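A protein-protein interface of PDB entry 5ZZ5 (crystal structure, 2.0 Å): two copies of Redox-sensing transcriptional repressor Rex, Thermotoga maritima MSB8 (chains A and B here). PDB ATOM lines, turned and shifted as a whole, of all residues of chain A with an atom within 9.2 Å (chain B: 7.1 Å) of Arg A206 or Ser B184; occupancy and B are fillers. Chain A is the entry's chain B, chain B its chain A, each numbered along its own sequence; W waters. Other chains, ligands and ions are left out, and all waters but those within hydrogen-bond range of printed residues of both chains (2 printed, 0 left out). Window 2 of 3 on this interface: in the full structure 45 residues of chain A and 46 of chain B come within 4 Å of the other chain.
The side-chain carboxylate (OE2) of Glu B166 sits at hydrogen-bond distance from the side-chain hydroxyl (OG) of Ser B184 (2.5 Å).
O of Pro B186 touches CD1 of Leu A199, 3.5 Å away. Ile A203 touches Lys B171 (CG1 to O, 3.5 Å). Ile A203 touches Gly B172 (CD1 to CA, 3.7 Å). Arg A206 touches Ser B184 (NH1 to O, 3.9 Å). NH1 of Arg A206 touches CA of Val B185 (3.8 Å). Arg A206 touches Pro B186.
Of chain A, only Arg A206 comes within 4 Å of Ser B184. Of chain A, only Arg A206 comes within 4 Å of Val B185. Of the printed residues of chain B, Ile A203 touches Lys B171 (3.5 Å) and Gly B172 (3.7 Å). Printed residues of chain B within 4 Å of Leu A199: Pro B186 (3.5 Å). Lys B182 touches none of the printed residues of chain A. Ile B170 touches none of the printed residues of chain A. The nearest residue of chain B that does not touch Arg A206 is Lys B171 (4.9 Å). The nearest printed residue of chain A that does not touch Pro B186 is Glu A202 (4.05 Å).
Of the 10 printed residues of chain A, 3 touch a printed residue of chain B. Hydrophobic or aromatic side chains of chain A within 4 Å of the printed part of chain B: Leu A199 and Ile A203. Of the 10 printed residues of chain B, 5 touch a printed residue of chain A. Hydrophobic or aromatic side chains of chain B that line the printed part of chain A: Pro B186.
No position is printed for both chains. Of the 6 pairs that touch across the chains among the printed residues, none has its exchanged pair printed and touching as well.
Water W2 bridges O of Lys B171 (2.7 Å) and NH1 of Arg A206 (2.9 Å). Water W1 lies within hydrogen-bond range of OG of Ser B184 and NH1 of Arg A206.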
ATOM      1  N   LEU A 199     -22.038  18.118 -20.001  1.00  0.00           N
ATOM      2  CA  LEU A 199     -21.792  18.247 -21.441  1.00  0.00           C
ATOM      3  C   LEU A 199     -20.640  19.201 -21.719  1.00  0.00           C
ATOM      4  O   LEU A 199     -19.737  18.874 -22.477  1.00  0.00           O
ATOM      5  CB  LEU A 199     -23.059  18.716 -22.188  1.00  0.00           C
ATOM      6  CG  LEU A 199     -22.947  18.944 -23.718  1.00  0.00           C
ATOM      7  CD1 LEU A 199     -22.598  17.654 -24.452  1.00  0.00           C
ATOM      8  CD2 LEU A 199     -24.233  19.508 -24.279  1.00  0.00           C
ATOM      9  N   THR A 200     -20.675  20.387 -21.114  1.00  0.00           N
ATOM     10  CA  THR A 200     -19.627  21.371 -21.356  1.00  0.00           C
ATOM     11  C   THR A 200     -18.273  20.930 -20.814  1.00  0.00           C
ATOM     12  O   THR A 200     -17.234  21.256 -21.395  1.00  0.00           O
ATOM     13  CB  THR A 200     -19.996  22.746 -20.783  1.00  0.00           C
ATOM     14  OG1 THR A 200     -20.419  22.600 -19.425  1.00  0.00           O
ATOM     15  CG2 THR A 200     -21.112  23.345 -21.590  1.00  0.00           C
ATOM     16  N   PHE A 201     -18.260  20.205 -19.701  1.00  0.00           N
ATOM     17  CA  PHE A 201     -16.979  19.685 -19.248  1.00  0.00           C
ATOM     18  C   PHE A 201     -16.372  18.777 -20.334  1.00  0.00           C
ATOM     19  O   PHE A 201     -15.186  18.868 -20.641  1.00  0.00           O
ATOM     20  CB  PHE A 201     -17.112  18.930 -17.937  1.00  0.00           C
ATOM     21  CG  PHE A 201     -15.822  18.404 -17.438  1.00  0.00           C
ATOM     22  CD1 PHE A 201     -14.879  19.260 -16.884  1.00  0.00           C
ATOM     23  CD2 PHE A 201     -15.508  17.063 -17.579  1.00  0.00           C
ATOM     24  CE1 PHE A 201     -13.664  18.778 -16.438  1.00  0.00           C
ATOM     25  CE2 PHE A 201     -14.287  16.577 -17.137  1.00  0.00           C
ATOM     26  CZ  PHE A 201     -13.371  17.438 -16.560  1.00  0.00           C
ATOM     27  N   GLU A 202     -17.201  17.921 -20.926  1.00  0.00           N
ATOM     28  CA  GLU A 202     -16.745  17.006 -21.959  1.00  0.00           C
ATOM     29  C   GLU A 202     -16.305  17.729 -23.234  1.00  0.00           C
ATOM     30  O   GLU A 202     -15.353  17.324 -23.881  1.00  0.00           O
ATOM     31  CB  GLU A 202     -17.843  15.991 -22.271  1.00  0.00           C
ATOM     32  CG  GLU A 202     -18.095  14.990 -21.147  1.00  0.00           C
ATOM     33  CD  GLU A 202     -16.895  14.084 -20.889  1.00  0.00           C
ATOM     34  OE1 GLU A 202     -16.076  13.905 -21.813  1.00  0.00           O
ATOM     35  OE2 GLU A 202     -16.770  13.553 -19.766  1.00  0.00           O
ATOM     36  N   ILE A 203     -16.994  18.802 -23.595  1.00  0.00           N
ATOM     37  CA  ILE A 203     -16.578  19.614 -24.730  1.00  0.00           C
ATOM     38  C   ILE A 203     -15.201  20.184 -24.491  1.00  0.00           C
ATOM     39  O   ILE A 203     -14.298  20.037 -25.328  1.00  0.00           O
ATOM     40  CB  ILE A 203     -17.559  20.768 -24.991  1.00  0.00           C
ATOM     41  CG1 ILE A 203     -18.877  20.224 -25.507  1.00  0.00           C
ATOM     42  CG2 ILE A 203     -16.992  21.757 -26.006  1.00  0.00           C
ATOM     43  CD1 ILE A 203     -19.937  21.329 -25.636  1.00  0.00           C
ATOM     44  N   VAL A 204     -15.034  20.831 -23.341  1.00  0.00           N
ATOM     45  CA  VAL A 204     -13.756  21.464 -23.036  1.00  0.00           C
ATOM     46  C   VAL A 204     -12.655  20.414 -22.902  1.00  0.00           C
ATOM     47  O   VAL A 204     -11.547  20.603 -23.386  1.00  0.00           O
ATOM     48  CB  VAL A 204     -13.825  22.322 -21.773  1.00  0.00           C
ATOM     49  CG1 VAL A 204     -12.442  22.782 -21.385  1.00  0.00           C
ATOM     50  CG2 VAL A 204     -14.727  23.534 -22.019  1.00  0.00           C
ATOM     51  N   ARG A 205     -12.987  19.284 -22.291  1.00  0.00           N
ATOM     52  CA  ARG A 205     -12.028  18.201 -22.110  1.00  0.00           C
ATOM     53  C   ARG A 205     -11.392  17.720 -23.439  1.00  0.00           C
ATOM     54  O   ARG A 205     -10.250  17.256 -23.451  1.00  0.00           O
ATOM     55  CB  ARG A 205     -12.687  17.032 -21.379  1.00  0.00           C
ATOM     56  CG  ARG A 205     -11.795  15.822 -21.282  1.00  0.00           C
ATOM     57  CD  ARG A 205     -12.389  14.737 -20.428  1.00  0.00           C
ATOM     58  NE  ARG A 205     -11.468  14.491 -19.323  1.00  0.00           N
ATOM     59  CZ  ARG A 205     -11.815  13.992 -18.144  1.00  0.00           C
ATOM     60  NH1 ARG A 205     -10.893  13.820 -17.206  1.00  0.00           N
ATOM     61  NH2 ARG A 205     -13.080  13.670 -17.901  1.00  0.00           N
ATOM     62  N   ARG A 206     -12.124  17.813 -24.546  1.00  0.00           N
ATOM     63  CA  ARG A 206     -11.601  17.372 -25.850  1.00  0.00           C
ATOM     64  C   ARG A 206     -10.410  18.201 -26.362  1.00  0.00           C
ATOM     65  O   ARG A 206      -9.651  17.740 -27.226  1.00  0.00           O
ATOM     66  CB  ARG A 206     -12.701  17.416 -26.912  1.00  0.00           C
ATOM     67  CG  ARG A 206     -13.768  16.322 -26.804  1.00  0.00           C
ATOM     68  CD  ARG A 206     -14.760  16.429 -27.966  1.00  0.00           C
ATOM     69  NE  ARG A 206     -14.203  15.908 -29.213  1.00  0.00           N
ATOM     70  CZ  ARG A 206     -14.685  16.171 -30.425  1.00  0.00           C
ATOM     71  NH1 ARG A 206     -15.730  16.980 -30.575  1.00  0.00           N
ATOM     72  NH2 ARG A 206     -14.103  15.644 -31.496  1.00  0.00           N
ATOM     73  N   ASN A 207     -10.197  19.381 -25.785  1.00  0.00           N
ATOM     74  CA  ASN A 207      -9.154  20.283 -26.265  1.00  0.00           C
ATOM     75  C   ASN A 207      -7.783  19.813 -25.771  1.00  0.00           C
ATOM     76  O   ASN A 207      -7.636  19.455 -24.606  1.00  0.00           O
ATOM     77  CB  ASN A 207      -9.417  21.706 -25.773  1.00  0.00           C
ATOM     78  CG  ASN A 207     -10.712  22.283 -26.323  1.00  0.00           C
ATOM     79  OD1 ASN A 207     -11.240  21.814 -27.339  1.00  0.00           O
ATOM     80  ND2 ASN A 207     -11.243  23.299 -25.638  1.00  0.00           N
ATOM     81  N   SER A 208      -6.805  19.740 -26.678  1.00  0.00           N
ATOM     82  CA  SER A 208      -5.457  19.296 -26.306  1.00  0.00           C
ATOM     83  C   SER A 208      -4.327  20.191 -26.838  1.00  0.00           C
ATOM     84  O   SER A 208      -4.547  21.338 -27.225  1.00  0.00           O
ATOM     85  CB  SER A 208      -5.228  17.852 -26.774  1.00  0.00           C
ATOM     86  OG  SER A 208      -5.156  17.770 -28.182  1.00  0.00           O
ATOM     87  N   GLU B 166     -24.224  19.081 -36.227  1.00  0.00           N
ATOM     88  CA  GLU B 166     -22.804  18.815 -36.277  1.00  0.00           C
ATOM     89  C   GLU B 166     -22.168  19.404 -37.542  1.00  0.00           C
ATOM     90  O   GLU B 166     -21.129  20.015 -37.469  1.00  0.00           O
ATOM     91  CB  GLU B 166     -22.590  17.300 -36.205  1.00  0.00           C
ATOM     92  CG  GLU B 166     -21.198  16.793 -36.473  1.00  0.00           C
ATOM     93  CD  GLU B 166     -21.163  15.273 -36.415  1.00  0.00           C
ATOM     94  OE1 GLU B 166     -21.936  14.625 -37.157  1.00  0.00           O
ATOM     95  OE2 GLU B 166     -20.402  14.731 -35.597  1.00  0.00           O
ATOM     96  N   ILE B 170     -21.771  22.727 -34.405  1.00  0.00           N
ATOM     97  CA  ILE B 170     -22.140  22.570 -32.989  1.00  0.00           C
ATOM     98  C   ILE B 170     -20.986  21.879 -32.261  1.00  0.00           C
ATOM     99  O   ILE B 170     -20.245  21.095 -32.860  1.00  0.00           O
ATOM    100  CB  ILE B 170     -23.466  21.762 -32.827  1.00  0.00           C
ATOM    101  CG1 ILE B 170     -24.287  22.260 -31.620  1.00  0.00           C
ATOM    102  CG2 ILE B 170     -23.178  20.260 -32.745  1.00  0.00           C
ATOM    103  CD1 ILE B 170     -24.878  23.660 -31.821  1.00  0.00           C
ATOM    104  N   LYS B 171     -20.796  22.207 -30.991  1.00  0.00           N
ATOM    105  CA  LYS B 171     -19.713  21.622 -30.217  1.00  0.00           C
ATOM    106  C   LYS B 171     -20.196  20.499 -29.293  1.00  0.00           C
ATOM    107  O   LYS B 171     -19.419  19.640 -28.876  1.00  0.00           O
ATOM    108  CB  LYS B 171     -19.045  22.725 -29.414  1.00  0.00           C
ATOM    109  CG  LYS B 171     -18.374  23.734 -30.343  1.00  0.00           C
ATOM    110  CD  LYS B 171     -17.901  24.978 -29.638  1.00  0.00           C
ATOM    111  CE  LYS B 171     -16.895  24.715 -28.546  1.00  0.00           C
ATOM    112  NZ  LYS B 171     -16.463  26.019 -27.942  1.00  0.00           N
ATOM    113  N   GLY B 172     -21.485  20.518 -28.978  1.00  0.00           N
ATOM    114  CA  GLY B 172     -22.072  19.518 -28.099  1.00  0.00           C
ATOM    115  C   GLY B 172     -23.576  19.487 -28.231  1.00  0.00           C
ATOM    116  O   GLY B 172     -24.193  20.463 -28.659  1.00  0.00           O
ATOM    117  N   LYS B 182     -25.838   9.252 -32.830  1.00  0.00           N
ATOM    118  CA  LYS B 182     -24.483   8.900 -33.247  1.00  0.00           C
ATOM    119  C   LYS B 182     -23.821  10.055 -33.998  1.00  0.00           C
ATOM    120  O   LYS B 182     -24.072  10.252 -35.176  1.00  0.00           O
ATOM    121  CB  LYS B 182     -24.525   7.648 -34.115  1.00  0.00           C
ATOM    122  CG  LYS B 182     -25.113   6.465 -33.367  1.00  0.00           C
ATOM    123  CD  LYS B 182     -25.437   5.309 -34.284  1.00  0.00           C
ATOM    124  CE  LYS B 182     -26.244   4.263 -33.532  1.00  0.00           C
ATOM    125  NZ  LYS B 182     -27.266   3.612 -34.394  1.00  0.00           N
ATOM    126  N   VAL B 183     -22.997  10.827 -33.297  1.00  0.00           N
ATOM    127  CA  VAL B 183     -22.315  11.973 -33.881  1.00  0.00           C
ATOM    128  C   VAL B 183     -20.907  12.008 -33.291  1.00  0.00           C
ATOM    129  O   VAL B 183     -20.625  11.260 -32.368  1.00  0.00           O
ATOM    130  CB  VAL B 183     -23.047  13.303 -33.586  1.00  0.00           C
ATOM    131  CG1 VAL B 183     -24.318  13.442 -34.416  1.00  0.00           C
ATOM    132  CG2 VAL B 183     -23.346  13.419 -32.112  1.00  0.00           C
ATOM    133  N   SER B 184     -20.025  12.868 -33.805  1.00  0.00           N
ATOM    134  CA  SER B 184     -18.657  12.941 -33.256  1.00  0.00           C
ATOM    135  C   SER B 184     -18.546  13.853 -32.024  1.00  0.00           C
ATOM    136  O   SER B 184     -17.651  13.666 -31.205  1.00  0.00           O
ATOM    137  CB  SER B 184     -17.647  13.369 -34.335  1.00  0.00           C
ATOM    138  OG  SER B 184     -18.009  14.587 -34.957  1.00  0.00           O
ATOM    139  N   VAL B 185     -19.414  14.862 -31.913  1.00  0.00           N
ATOM    140  CA  VAL B 185     -19.377  15.782 -30.764  1.00  0.00           C
ATOM    141  C   VAL B 185     -19.936  15.109 -29.500  1.00  0.00           C
ATOM    142  O   VAL B 185     -20.686  14.150 -29.601  1.00  0.00           O
ATOM    143  CB  VAL B 185     -20.184  17.072 -31.051  1.00  0.00           C
ATOM    144  CG1 VAL B 185     -19.565  17.829 -32.251  1.00  0.00           C
ATOM    145  CG2 VAL B 185     -21.638  16.732 -31.323  1.00  0.00           C
ATOM    146  N   PRO B 186     -19.579  15.609 -28.302  1.00  0.00           N
ATOM    147  CA  PRO B 186     -20.193  15.001 -27.116  1.00  0.00           C
ATOM    148  C   PRO B 186     -21.717  15.167 -27.095  1.00  0.00           C
ATOM    149  O   PRO B 186     -22.264  16.161 -27.606  1.00  0.00           O
ATOM    150  CB  PRO B 186     -19.541  15.760 -25.959  1.00  0.00           C
ATOM    151  CG  PRO B 186     -18.220  16.168 -26.492  1.00  0.00           C
ATOM    152  CD  PRO B 186     -18.470  16.512 -27.942  1.00  0.00           C
ATOM    153  N   VAL B 187     -22.381  14.169 -26.517  1.00  0.00           N
ATOM    154  CA  VAL B 187     -23.827  14.135 -26.370  1.00  0.00           C
ATOM    155  C   VAL B 187     -24.140  13.824 -24.913  1.00  0.00           C
ATOM    156  O   VAL B 187     -23.526  12.933 -24.332  1.00  0.00           O
ATOM    157  CB  VAL B 187     -24.480  13.047 -27.274  1.00  0.00           C
ATOM    158  CG1 VAL B 187     -25.999  13.002 -27.069  1.00  0.00           C
ATOM    159  CG2 VAL B 187     -24.173  13.302 -28.740  1.00  0.00           C
HETATM  160  O   HOH W   1     -16.473  16.843 -33.724  1.00  0.00           O
HETATM  161  O   HOH W   2     -16.812  19.444 -29.598  1.00  0.00           O
